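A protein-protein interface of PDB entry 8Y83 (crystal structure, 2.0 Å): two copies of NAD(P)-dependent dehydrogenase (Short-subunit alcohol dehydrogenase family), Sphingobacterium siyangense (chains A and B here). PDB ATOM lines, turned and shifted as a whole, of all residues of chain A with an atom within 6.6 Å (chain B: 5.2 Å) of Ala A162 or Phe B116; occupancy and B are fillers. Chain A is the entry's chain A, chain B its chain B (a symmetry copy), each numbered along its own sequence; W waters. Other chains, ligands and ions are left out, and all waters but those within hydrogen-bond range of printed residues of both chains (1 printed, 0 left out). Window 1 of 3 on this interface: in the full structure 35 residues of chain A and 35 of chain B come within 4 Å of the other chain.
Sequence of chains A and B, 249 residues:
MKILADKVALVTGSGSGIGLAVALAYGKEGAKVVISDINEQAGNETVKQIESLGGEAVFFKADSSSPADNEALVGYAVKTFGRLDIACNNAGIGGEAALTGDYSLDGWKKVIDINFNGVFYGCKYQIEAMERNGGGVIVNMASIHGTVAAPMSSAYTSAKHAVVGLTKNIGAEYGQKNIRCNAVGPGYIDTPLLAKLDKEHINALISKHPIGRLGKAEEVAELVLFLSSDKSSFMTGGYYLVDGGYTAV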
ATOM      1  N   TRP A 108     -11.859  18.112  22.851  1.00  0.00           N
ATOM      2  CA  TRP A 108     -11.812  19.563  22.952  1.00  0.00           C
ATOM      3  C   TRP A 108     -10.399  20.087  22.687  1.00  0.00           C
ATOM      4  O   TRP A 108     -10.183  20.956  21.839  1.00  0.00           O
ATOM      5  CB  TRP A 108     -12.301  20.026  24.338  1.00  0.00           C
ATOM      6  CG  TRP A 108     -12.210  21.520  24.523  1.00  0.00           C
ATOM      7  CD1 TRP A 108     -11.142  22.208  25.012  1.00  0.00           C
ATOM      8  CD2 TRP A 108     -13.224  22.512  24.232  1.00  0.00           C
ATOM      9  NE1 TRP A 108     -11.396  23.559  25.010  1.00  0.00           N
ATOM     10  CE2 TRP A 108     -12.664  23.776  24.530  1.00  0.00           C
ATOM     11  CE3 TRP A 108     -14.537  22.462  23.754  1.00  0.00           C
ATOM     12  CZ2 TRP A 108     -13.369  24.975  24.336  1.00  0.00           C
ATOM     13  CZ3 TRP A 108     -15.238  23.635  23.568  1.00  0.00           C
ATOM     14  CH2 TRP A 108     -14.662  24.873  23.863  1.00  0.00           C
ATOM     15  N   ILE A 112      -8.976  22.542  19.637  1.00  0.00           N
ATOM     16  CA  ILE A 112      -8.411  23.842  19.956  1.00  0.00           C
ATOM     17  C   ILE A 112      -6.945  23.926  19.497  1.00  0.00           C
ATOM     18  O   ILE A 112      -6.507  24.960  18.974  1.00  0.00           O
ATOM     19  CB  ILE A 112      -8.578  24.140  21.462  1.00  0.00           C
ATOM     20  CG1 ILE A 112     -10.054  24.188  21.928  1.00  0.00           C
ATOM     21  CG2 ILE A 112      -7.802  25.387  21.883  1.00  0.00           C
ATOM     22  CD1 ILE A 112     -11.064  24.695  20.930  1.00  0.00           C
ATOM     23  N   PHE A 116      -7.009  26.383  16.393  1.00  0.00           N
ATOM     24  CA  PHE A 116      -6.815  27.677  16.998  1.00  0.00           C
ATOM     25  C   PHE A 116      -5.329  27.895  17.313  1.00  0.00           C
ATOM     26  O   PHE A 116      -4.738  28.844  16.759  1.00  0.00           O
ATOM     27  CB  PHE A 116      -7.698  27.967  18.208  1.00  0.00           C
ATOM     28  CG  PHE A 116      -7.322  29.311  18.807  1.00  0.00           C
ATOM     29  CD1 PHE A 116      -7.175  30.442  18.002  1.00  0.00           C
ATOM     30  CD2 PHE A 116      -7.000  29.407  20.138  1.00  0.00           C
ATOM     31  CE1 PHE A 116      -6.733  31.635  18.547  1.00  0.00           C
ATOM     32  CE2 PHE A 116      -6.594  30.603  20.680  1.00  0.00           C
ATOM     33  CZ  PHE A 116      -6.455  31.709  19.886  1.00  0.00           C
ATOM     34  N   ASN A 117      -4.780  27.143  18.286  1.00  0.00           N
ATOM     35  CA  ASN A 117      -3.388  27.344  18.698  1.00  0.00           C
ATOM     36  C   ASN A 117      -2.434  27.240  17.508  1.00  0.00           C
ATOM     37  O   ASN A 117      -1.501  28.046  17.358  1.00  0.00           O
ATOM     38  CB  ASN A 117      -2.932  26.418  19.826  1.00  0.00           C
ATOM     39  CG  ASN A 117      -3.551  26.826  21.146  1.00  0.00           C
ATOM     40  OD1 ASN A 117      -3.739  28.018  21.419  1.00  0.00           O
ATOM     41  ND2 ASN A 117      -4.008  25.862  21.925  1.00  0.00           N
ATOM     42  N   GLY A 146     -17.289  30.828  12.798  1.00  0.00           N
ATOM     43  CA  GLY A 146     -16.680  31.987  13.422  1.00  0.00           C
ATOM     44  C   GLY A 146     -17.682  33.055  13.866  1.00  0.00           C
ATOM     45  O   GLY A 146     -17.297  34.003  14.558  1.00  0.00           O
ATOM     46  N   SER A 154     -19.148  22.530  19.670  1.00  0.00           N
ATOM     47  CA  SER A 154     -18.726  23.694  20.445  1.00  0.00           C
ATOM     48  C   SER A 154     -17.233  24.000  20.311  1.00  0.00           C
ATOM     49  O   SER A 154     -16.835  25.178  20.327  1.00  0.00           O
ATOM     50  CB  SER A 154     -19.149  23.538  21.889  1.00  0.00           C
ATOM     51  OG  SER A 154     -18.538  22.349  22.382  1.00  0.00           O
ATOM     52  N   ALA A 155     -16.365  22.977  20.259  1.00  0.00           N
ATOM     53  CA  ALA A 155     -14.939  23.282  20.166  1.00  0.00           C
ATOM     54  C   ALA A 155     -14.609  23.927  18.821  1.00  0.00           C
ATOM     55  O   ALA A 155     -13.822  24.856  18.759  1.00  0.00           O
ATOM     56  CB  ALA A 155     -14.063  22.054  20.411  1.00  0.00           C
ATOM     57  N   THR A 157     -16.726  25.739  16.835  1.00  0.00           N
ATOM     58  CA  THR A 157     -17.273  27.095  16.869  1.00  0.00           C
ATOM     59  C   THR A 157     -16.353  27.997  17.686  1.00  0.00           C
ATOM     60  O   THR A 157     -16.016  29.075  17.268  1.00  0.00           O
ATOM     61  CB  THR A 157     -18.693  27.082  17.439  1.00  0.00           C
ATOM     62  OG1 THR A 157     -19.445  26.134  16.681  1.00  0.00           O
ATOM     63  CG2 THR A 157     -19.328  28.460  17.456  1.00  0.00           C
ATOM     64  N   SER A 158     -15.964  27.560  18.889  1.00  0.00           N
ATOM     65  CA  SER A 158     -15.091  28.333  19.753  1.00  0.00           C
ATOM     66  C   SER A 158     -13.751  28.669  19.063  1.00  0.00           C
ATOM     67  O   SER A 158     -13.285  29.828  19.109  1.00  0.00           O
ATOM     68  CB  SER A 158     -14.883  27.606  21.047  1.00  0.00           C
ATOM     69  OG  SER A 158     -16.127  27.402  21.693  1.00  0.00           O
ATOM     70  N   ALA A 159     -13.121  27.645  18.463  1.00  0.00           N
ATOM     71  CA  ALA A 159     -11.843  27.827  17.806  1.00  0.00           C
ATOM     72  C   ALA A 159     -11.955  28.802  16.625  1.00  0.00           C
ATOM     73  O   ALA A 159     -11.055  29.610  16.410  1.00  0.00           O
ATOM     74  CB  ALA A 159     -11.304  26.477  17.352  1.00  0.00           C
ATOM     75  N   LYS A 160     -13.014  28.672  15.821  1.00  0.00           N
ATOM     76  CA  LYS A 160     -13.188  29.505  14.634  1.00  0.00           C
ATOM     77  C   LYS A 160     -13.488  30.957  15.018  1.00  0.00           C
ATOM     78  O   LYS A 160     -13.025  31.876  14.338  1.00  0.00           O
ATOM     79  CB  LYS A 160     -14.260  28.901  13.731  1.00  0.00           C
ATOM     80  CG  LYS A 160     -13.853  27.580  13.141  1.00  0.00           C
ATOM     81  CD  LYS A 160     -12.563  27.599  12.345  1.00  0.00           C
ATOM     82  CE  LYS A 160     -12.384  26.399  11.480  1.00  0.00           C
ATOM     83  NZ  LYS A 160     -11.213  26.533  10.574  1.00  0.00           N
ATOM     84  N   HIS A 161     -14.250  31.143  16.104  1.00  0.00           N
ATOM     85  CA  HIS A 161     -14.404  32.456  16.716  1.00  0.00           C
ATOM     86  C   HIS A 161     -13.047  33.042  17.098  1.00  0.00           C
ATOM     87  O   HIS A 161     -12.777  34.206  16.778  1.00  0.00           O
ATOM     88  CB  HIS A 161     -15.359  32.447  17.921  1.00  0.00           C
ATOM     89  CG  HIS A 161     -16.795  32.629  17.592  1.00  0.00           C
ATOM     90  ND1 HIS A 161     -17.540  31.682  16.908  1.00  0.00           N
ATOM     91  CD2 HIS A 161     -17.633  33.634  17.878  1.00  0.00           C
ATOM     92  CE1 HIS A 161     -18.795  32.118  16.801  1.00  0.00           C
ATOM     93  NE2 HIS A 161     -18.870  33.306  17.395  1.00  0.00           N
ATOM     94  N   ALA A 162     -12.222  32.237  17.789  1.00  0.00           N
ATOM     95  CA  ALA A 162     -10.891  32.660  18.221  1.00  0.00           C
ATOM     96  C   ALA A 162      -9.976  33.049  17.054  1.00  0.00           C
ATOM     97  O   ALA A 162      -9.225  34.031  17.139  1.00  0.00           O
ATOM     98  CB  ALA A 162     -10.277  31.608  19.103  1.00  0.00           C
ATOM     99  N   VAL A 163     -10.073  32.353  15.929  1.00  0.00           N
ATOM    100  CA  VAL A 163      -9.346  32.720  14.716  1.00  0.00           C
ATOM    101  C   VAL A 163      -9.748  34.102  14.185  1.00  0.00           C
ATOM    102  O   VAL A 163      -8.892  34.849  13.663  1.00  0.00           O
ATOM    103  CB  VAL A 163      -9.527  31.653  13.620  1.00  0.00           C
ATOM    104  CG1 VAL A 163      -9.041  32.124  12.256  1.00  0.00           C
ATOM    105  CG2 VAL A 163      -8.886  30.322  14.001  1.00  0.00           C
ATOM    106  N   VAL A 164     -11.052  34.415  14.247  1.00  0.00           N
ATOM    107  CA  VAL A 164     -11.522  35.742  13.854  1.00  0.00           C
ATOM    108  C   VAL A 164     -10.909  36.821  14.767  1.00  0.00           C
ATOM    109  O   VAL A 164     -10.461  37.844  14.255  1.00  0.00           O
ATOM    110  CB  VAL A 164     -13.055  35.783  13.842  1.00  0.00           C
ATOM    111  CG1 VAL A 164     -13.588  37.203  13.686  1.00  0.00           C
ATOM    112  CG2 VAL A 164     -13.645  34.846  12.769  1.00  0.00           C
ATOM    113  N   GLY A 165     -10.904  36.610  16.098  1.00  0.00           N
ATOM    114  CA  GLY A 165     -10.279  37.554  17.019  1.00  0.00           C
ATOM    115  C   GLY A 165      -8.784  37.752  16.732  1.00  0.00           C
ATOM    116  O   GLY A 165      -8.295  38.881  16.703  1.00  0.00           O
ATOM    117  N   LEU A 166      -8.060  36.629  16.543  1.00  0.00           N
ATOM    118  CA  LEU A 166      -6.643  36.665  16.272  1.00  0.00           C
ATOM    119  C   LEU A 166      -6.408  37.500  15.012  1.00  0.00           C
ATOM    120  O   LEU A 166      -5.498  38.325  14.961  1.00  0.00           O
ATOM    121  CB  LEU A 166      -6.118  35.235  16.150  1.00  0.00           C
ATOM    122  CG  LEU A 166      -4.672  35.095  15.673  1.00  0.00           C
ATOM    123  CD1 LEU A 166      -3.685  35.719  16.631  1.00  0.00           C
ATOM    124  CD2 LEU A 166      -4.321  33.635  15.389  1.00  0.00           C
ATOM    125  N   THR A 167      -7.235  37.275  13.992  1.00  0.00           N
ATOM    126  CA  THR A 167      -7.111  37.976  12.724  1.00  0.00           C
ATOM    127  C   THR A 167      -7.256  39.485  12.933  1.00  0.00           C
ATOM    128  O   THR A 167      -6.513  40.285  12.361  1.00  0.00           O
ATOM    129  CB  THR A 167      -8.177  37.440  11.771  1.00  0.00           C
ATOM    130  OG1 THR A 167      -7.909  36.043  11.568  1.00  0.00           O
ATOM    131  CG2 THR A 167      -8.164  38.235  10.476  1.00  0.00           C
ATOM    132  N   VAL B 111      -2.788  32.283  28.914  1.00  0.00           N
ATOM    133  CA  VAL B 111      -3.991  33.069  28.667  1.00  0.00           C
ATOM    134  C   VAL B 111      -5.073  32.187  28.036  1.00  0.00           C
ATOM    135  O   VAL B 111      -6.207  32.204  28.481  1.00  0.00           O
ATOM    136  CB  VAL B 111      -3.704  34.314  27.805  1.00  0.00           C
ATOM    137  CG1 VAL B 111      -4.976  35.032  27.370  1.00  0.00           C
ATOM    138  CG2 VAL B 111      -2.765  35.286  28.514  1.00  0.00           C
ATOM    139  N   ILE B 112      -4.725  31.347  27.063  1.00  0.00           N
ATOM    140  CA  ILE B 112      -5.714  30.485  26.431  1.00  0.00           C
ATOM    141  C   ILE B 112      -6.291  29.509  27.463  1.00  0.00           C
ATOM    142  O   ILE B 112      -7.509  29.295  27.504  1.00  0.00           O
ATOM    143  CB  ILE B 112      -5.141  29.791  25.177  1.00  0.00           C
ATOM    144  CG1 ILE B 112      -4.682  30.821  24.122  1.00  0.00           C
ATOM    145  CG2 ILE B 112      -6.121  28.781  24.586  1.00  0.00           C
ATOM    146  CD1 ILE B 112      -5.684  31.916  23.804  1.00  0.00           C
ATOM    147  N   ASP B 113      -5.418  28.950  28.314  1.00  0.00           N
ATOM    148  CA  ASP B 113      -5.838  27.950  29.282  1.00  0.00           C
ATOM    149  C   ASP B 113      -6.825  28.521  30.275  1.00  0.00           C
ATOM    150  O   ASP B 113      -7.765  27.816  30.626  1.00  0.00           O
ATOM    151  CB  ASP B 113      -4.673  27.269  29.987  1.00  0.00           C
ATOM    152  CG  ASP B 113      -3.993  26.203  29.141  1.00  0.00           C
ATOM    153  OD1 ASP B 113      -4.565  25.854  28.084  1.00  0.00           O
ATOM    154  OD2 ASP B 113      -2.884  25.763  29.506  1.00  0.00           O
ATOM    155  N   ILE B 114      -6.589  29.749  30.764  1.00  0.00           N
ATOM    156  CA  ILE B 114      -7.448  30.311  31.791  1.00  0.00           C
ATOM    157  C   ILE B 114      -8.717  30.874  31.147  1.00  0.00           C
ATOM    158  O   ILE B 114      -9.830  30.553  31.591  1.00  0.00           O
ATOM    159  CB  ILE B 114      -6.699  31.343  32.673  1.00  0.00           C
ATOM    160  CG1 ILE B 114      -5.531  30.681  33.423  1.00  0.00           C
ATOM    161  CG2 ILE B 114      -7.665  32.054  33.631  1.00  0.00           C
ATOM    162  CD1 ILE B 114      -4.588  31.664  34.090  1.00  0.00           C
ATOM    163  N   ASN B 115      -8.527  31.720  30.116  1.00  0.00           N
ATOM    164  CA  ASN B 115      -9.600  32.557  29.586  1.00  0.00           C
ATOM    165  C   ASN B 115     -10.503  31.817  28.586  1.00  0.00           C
ATOM    166  O   ASN B 115     -11.621  32.261  28.367  1.00  0.00           O
ATOM    167  CB  ASN B 115      -9.060  33.833  28.941  1.00  0.00           C
ATOM    168  CG  ASN B 115      -8.413  34.771  29.936  1.00  0.00           C
ATOM    169  OD1 ASN B 115      -8.045  34.375  31.043  1.00  0.00           O
ATOM    170  ND2 ASN B 115      -8.202  36.014  29.543  1.00  0.00           N
ATOM    171  N   PHE B 116     -10.023  30.744  27.944  1.00  0.00           N
ATOM    172  CA  PHE B 116     -10.780  30.033  26.906  1.00  0.00           C
ATOM    173  C   PHE B 116     -11.114  28.627  27.420  1.00  0.00           C
ATOM    174  O   PHE B 116     -12.261  28.324  27.716  1.00  0.00           O
ATOM    175  CB  PHE B 116      -9.923  30.122  25.633  1.00  0.00           C
ATOM    176  CG  PHE B 116     -10.302  29.396  24.331  1.00  0.00           C
ATOM    177  CD1 PHE B 116     -11.347  28.485  24.277  1.00  0.00           C
ATOM    178  CD2 PHE B 116      -9.628  29.688  23.131  1.00  0.00           C
ATOM    179  CE1 PHE B 116     -11.688  27.861  23.090  1.00  0.00           C
ATOM    180  CE2 PHE B 116      -9.966  29.054  21.928  1.00  0.00           C
ATOM    181  CZ  PHE B 116     -10.998  28.130  21.914  1.00  0.00           C
ATOM    182  N   ASN B 117     -10.094  27.770  27.524  1.00  0.00           N
ATOM    183  CA  ASN B 117     -10.288  26.380  27.932  1.00  0.00           C
ATOM    184  C   ASN B 117     -11.001  26.279  29.281  1.00  0.00           C
ATOM    185  O   ASN B 117     -11.922  25.470  29.444  1.00  0.00           O
ATOM    186  CB  ASN B 117      -8.974  25.608  27.952  1.00  0.00           C
ATOM    187  CG  ASN B 117      -8.387  25.430  26.569  1.00  0.00           C
ATOM    188  OD1 ASN B 117      -9.101  25.235  25.574  1.00  0.00           O
ATOM    189  ND2 ASN B 117      -7.078  25.537  26.487  1.00  0.00           N
ATOM    190  N   GLY B 118     -10.594  27.124  30.234  1.00  0.00           N
ATOM    191  CA  GLY B 118     -11.175  27.117  31.554  1.00  0.00           C
ATOM    192  C   GLY B 118     -12.666  27.444  31.566  1.00  0.00           C
ATOM    193  O   GLY B 118     -13.417  26.859  32.337  1.00  0.00           O
ATOM    194  N   VAL B 119     -13.113  28.368  30.704  1.00  0.00           N
ATOM    195  CA  VAL B 119     -14.529  28.692  30.639  1.00  0.00           C
ATOM    196  C   VAL B 119     -15.280  27.464  30.138  1.00  0.00           C
ATOM    197  O   VAL B 119     -16.382  27.162  30.585  1.00  0.00           O
ATOM    198  CB  VAL B 119     -14.759  29.945  29.756  1.00  0.00           C
ATOM    199  CG1 VAL B 119     -16.221  30.259  29.563  1.00  0.00           C
ATOM    200  CG2 VAL B 119     -14.057  31.175  30.334  1.00  0.00           C
ATOM    201  N   PHE B 120     -14.705  26.763  29.169  1.00  0.00           N
ATOM    202  CA  PHE B 120     -15.352  25.553  28.694  1.00  0.00           C
ATOM    203  C   PHE B 120     -15.421  24.505  29.810  1.00  0.00           C
ATOM    204  O   PHE B 120     -16.457  23.870  30.004  1.00  0.00           O
ATOM    205  CB  PHE B 120     -14.666  24.957  27.465  1.00  0.00           C
ATOM    206  CG  PHE B 120     -14.981  23.476  27.261  1.00  0.00           C
ATOM    207  CD1 PHE B 120     -16.243  23.061  26.885  1.00  0.00           C
ATOM    208  CD2 PHE B 120     -14.003  22.506  27.478  1.00  0.00           C
ATOM    209  CE1 PHE B 120     -16.519  21.717  26.711  1.00  0.00           C
ATOM    210  CE2 PHE B 120     -14.268  21.166  27.294  1.00  0.00           C
ATOM    211  CZ  PHE B 120     -15.514  20.776  26.881  1.00  0.00           C
ATOM    212  N   SER B 158      -8.427  36.697  21.371  1.00  0.00           N
ATOM    213  CA  SER B 158      -8.765  35.423  20.779  1.00  0.00           C
ATOM    214  C   SER B 158      -9.637  34.609  21.729  1.00  0.00           C
ATOM    215  O   SER B 158     -10.669  34.087  21.322  1.00  0.00           O
ATOM    216  CB  SER B 158      -7.567  34.637  20.381  1.00  0.00           C
ATOM    217  OG  SER B 158      -6.727  35.301  19.452  1.00  0.00           O
ATOM    218  N   ALA B 159      -9.232  34.549  22.992  1.00  0.00           N
ATOM    219  CA  ALA B 159      -9.961  33.802  23.997  1.00  0.00           C
ATOM    220  C   ALA B 159     -11.346  34.401  24.251  1.00  0.00           C
ATOM    221  O   ALA B 159     -12.313  33.666  24.415  1.00  0.00           O
ATOM    222  CB  ALA B 159      -9.148  33.772  25.267  1.00  0.00           C
ATOM    223  N   HIS B 161     -13.199  36.230  22.047  1.00  0.00           N
ATOM    224  CA  HIS B 161     -13.980  35.763  20.895  1.00  0.00           C
ATOM    225  C   HIS B 161     -14.473  34.318  21.071  1.00  0.00           C
ATOM    226  O   HIS B 161     -15.635  34.046  20.782  1.00  0.00           O
ATOM    227  CB  HIS B 161     -13.151  35.864  19.617  1.00  0.00           C
ATOM    228  CG  HIS B 161     -13.167  37.206  18.979  1.00  0.00           C
ATOM    229  ND1 HIS B 161     -12.607  38.313  19.578  1.00  0.00           N
ATOM    230  CD2 HIS B 161     -13.664  37.618  17.815  1.00  0.00           C
ATOM    231  CE1 HIS B 161     -12.803  39.365  18.776  1.00  0.00           C
ATOM    232  NE2 HIS B 161     -13.443  38.967  17.701  1.00  0.00           N
ATOM    233  N   ALA B 162     -13.597  33.406  21.562  1.00  0.00           N
ATOM    234  CA  ALA B 162     -13.940  31.994  21.755  1.00  0.00           C
ATOM    235  C   ALA B 162     -15.100  31.842  22.730  1.00  0.00           C
ATOM    236  O   ALA B 162     -16.026  31.058  22.506  1.00  0.00           O
ATOM    237  CB  ALA B 162     -12.729  31.183  22.246  1.00  0.00           C
ATOM    238  N   VAL B 163     -15.077  32.642  23.790  1.00  0.00           N
ATOM    239  CA  VAL B 163     -16.122  32.600  24.799  1.00  0.00           C
ATOM    240  C   VAL B 163     -17.480  32.983  24.183  1.00  0.00           C
ATOM    241  O   VAL B 163     -18.520  32.406  24.504  1.00  0.00           O
ATOM    242  CB  VAL B 163     -15.741  33.510  25.989  1.00  0.00           C
ATOM    243  CG1 VAL B 163     -16.914  33.761  26.907  1.00  0.00           C
ATOM    244  CG2 VAL B 163     -14.538  33.011  26.797  1.00  0.00           C
ATOM    245  N   LEU B 166     -18.620  29.930  22.184  1.00  0.00           N
ATOM    246  CA  LEU B 166     -19.040  28.868  23.091  1.00  0.00           C
ATOM    247  C   LEU B 166     -20.429  29.133  23.639  1.00  0.00           C
ATOM    248  O   LEU B 166     -21.245  28.218  23.782  1.00  0.00           O
ATOM    249  CB  LEU B 166     -17.991  28.769  24.192  1.00  0.00           C
ATOM    250  CG  LEU B 166     -18.327  27.820  25.349  1.00  0.00           C
ATOM    251  CD1 LEU B 166     -18.492  26.404  24.863  1.00  0.00           C
ATOM    252  CD2 LEU B 166     -17.195  27.930  26.390  1.00  0.00           C
HETATM  253  O   HOH W   1      -5.287  23.759  24.302  1.00  0.00           O
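Hydrophobic or aromatic side chains of chain A that line the printed part of chain B: Trp A108, Ile A112, Phe A116, His A161, Ala A162 and Leu A166. Of the 16 printed residues of chain B, 8 touch a printed residue of chain A. Hydrophobic or aromatic side chains of chain B within 4 Å of the printed part of chain A: Ile B112, Phe B116, Phe B120, His B161, Ala B162 and Leu B166. Among the printed residues, 16 pairs touch across the chains. Among the printed residues, no Asp or Glu carboxylate lies within 4 Å of a Lys or Arg side-chain nitrogen of the other chain.
Water W1 bridges the side-chain amide nitrogen of Asn B117 and the side-chain amide nitrogen of Asn A117.
Among the printed residues, pairs that only touch across the chains: Trp A108 with Phe B116, Trp A108 with Phe B120, Ile A112 with Phe B116, Ile A112 with Asn B117, Phe A116 with Ile B112, Phe A116 with Phe B116, Phe A116 with Ser B158, Ser A158 with Phe B116, Ser A158 with Ala B162, Ser A158 with Leu B166, His A161 with His B161, Ala A162 with Phe B116, Ala A162 with Ser B158 and Gly A165 with His B161.
Of the printed residues of chain B, Ser A158 touches Phe B116, Ala B162 and Leu B166. Of the printed residues of chain B, Ala A162 touches Phe B116 and Ser B158. Phe B116 touches just these residues of chain A: Trp A108 (3.6 Å), Ile A112 (3.6 Å), Phe A116 (3.5 Å), Ser A158 (3.8 Å) and Ala A162 (3.8 Å). Of the printed residues of chain A, Ala B162 touches Ser A158 (3.5 Å). Printed residues of chain A within 4 Å of Leu B166: Ser A158. The nearest printed residue of chain B that does not touch Ala A162 is Ala B162 (4.01 Å). The nearest residue of chain A that does not touch Phe B116 is Ala A159 (4.1 Å). The nearest printed residue of chain B that does not touch Ser A158 is His B161 (5.0 Å).
The backbone carbonyl oxygen of Ile A112 sits at hydrogen-bond distance from the backbone NH of Asn A117 (2.9 Å). A ring nitrogen (ND1) of His A161 lies close to the backbone carbonyl oxygen of Gly A146, at 3.3 Å. O of Ser A154 lies within hydrogen-bond range of OG of Ser A158, at 2.7 Å. ND1 of His A161 is in hydrogen-bond range of O of Thr A157, 3.0 Å away. The backbone carbonyl oxygen (O) of Ile B112 lies within hydrogen-bond range of the backbone NH (N) of Asn B117, 3.0 Å away. OD1 of Asp B113 is in hydrogen-bond range of ND2 of Asn B117 (3.0 Å).
The side-chain amide oxygen (OD1) of Asn B117 sits at hydrogen-bond distance from the indole nitrogen (NE1) of Trp A108 (2.9 Å). N of Leu A166 sits close to OG of Ser B158.
Ile A112 touches Asn B117, but with the chains exchanged Asn A117 does not touch Ile B112 (4.01 Å). Phe B116 touches its own counterpart, Phe A116. Phe A116 touches Ser B158, and with the chains exchanged Ser A158 touches Phe B116. Ala A162 touches Phe B116, but with the chains exchanged Phe A116 does not touch Ala B162 (6.4 Å). 9 positions are printed for both chains. Of the 16 pairs that touch across the chains among the printed residues, 10 have their exchanged pair printed and touching as well.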
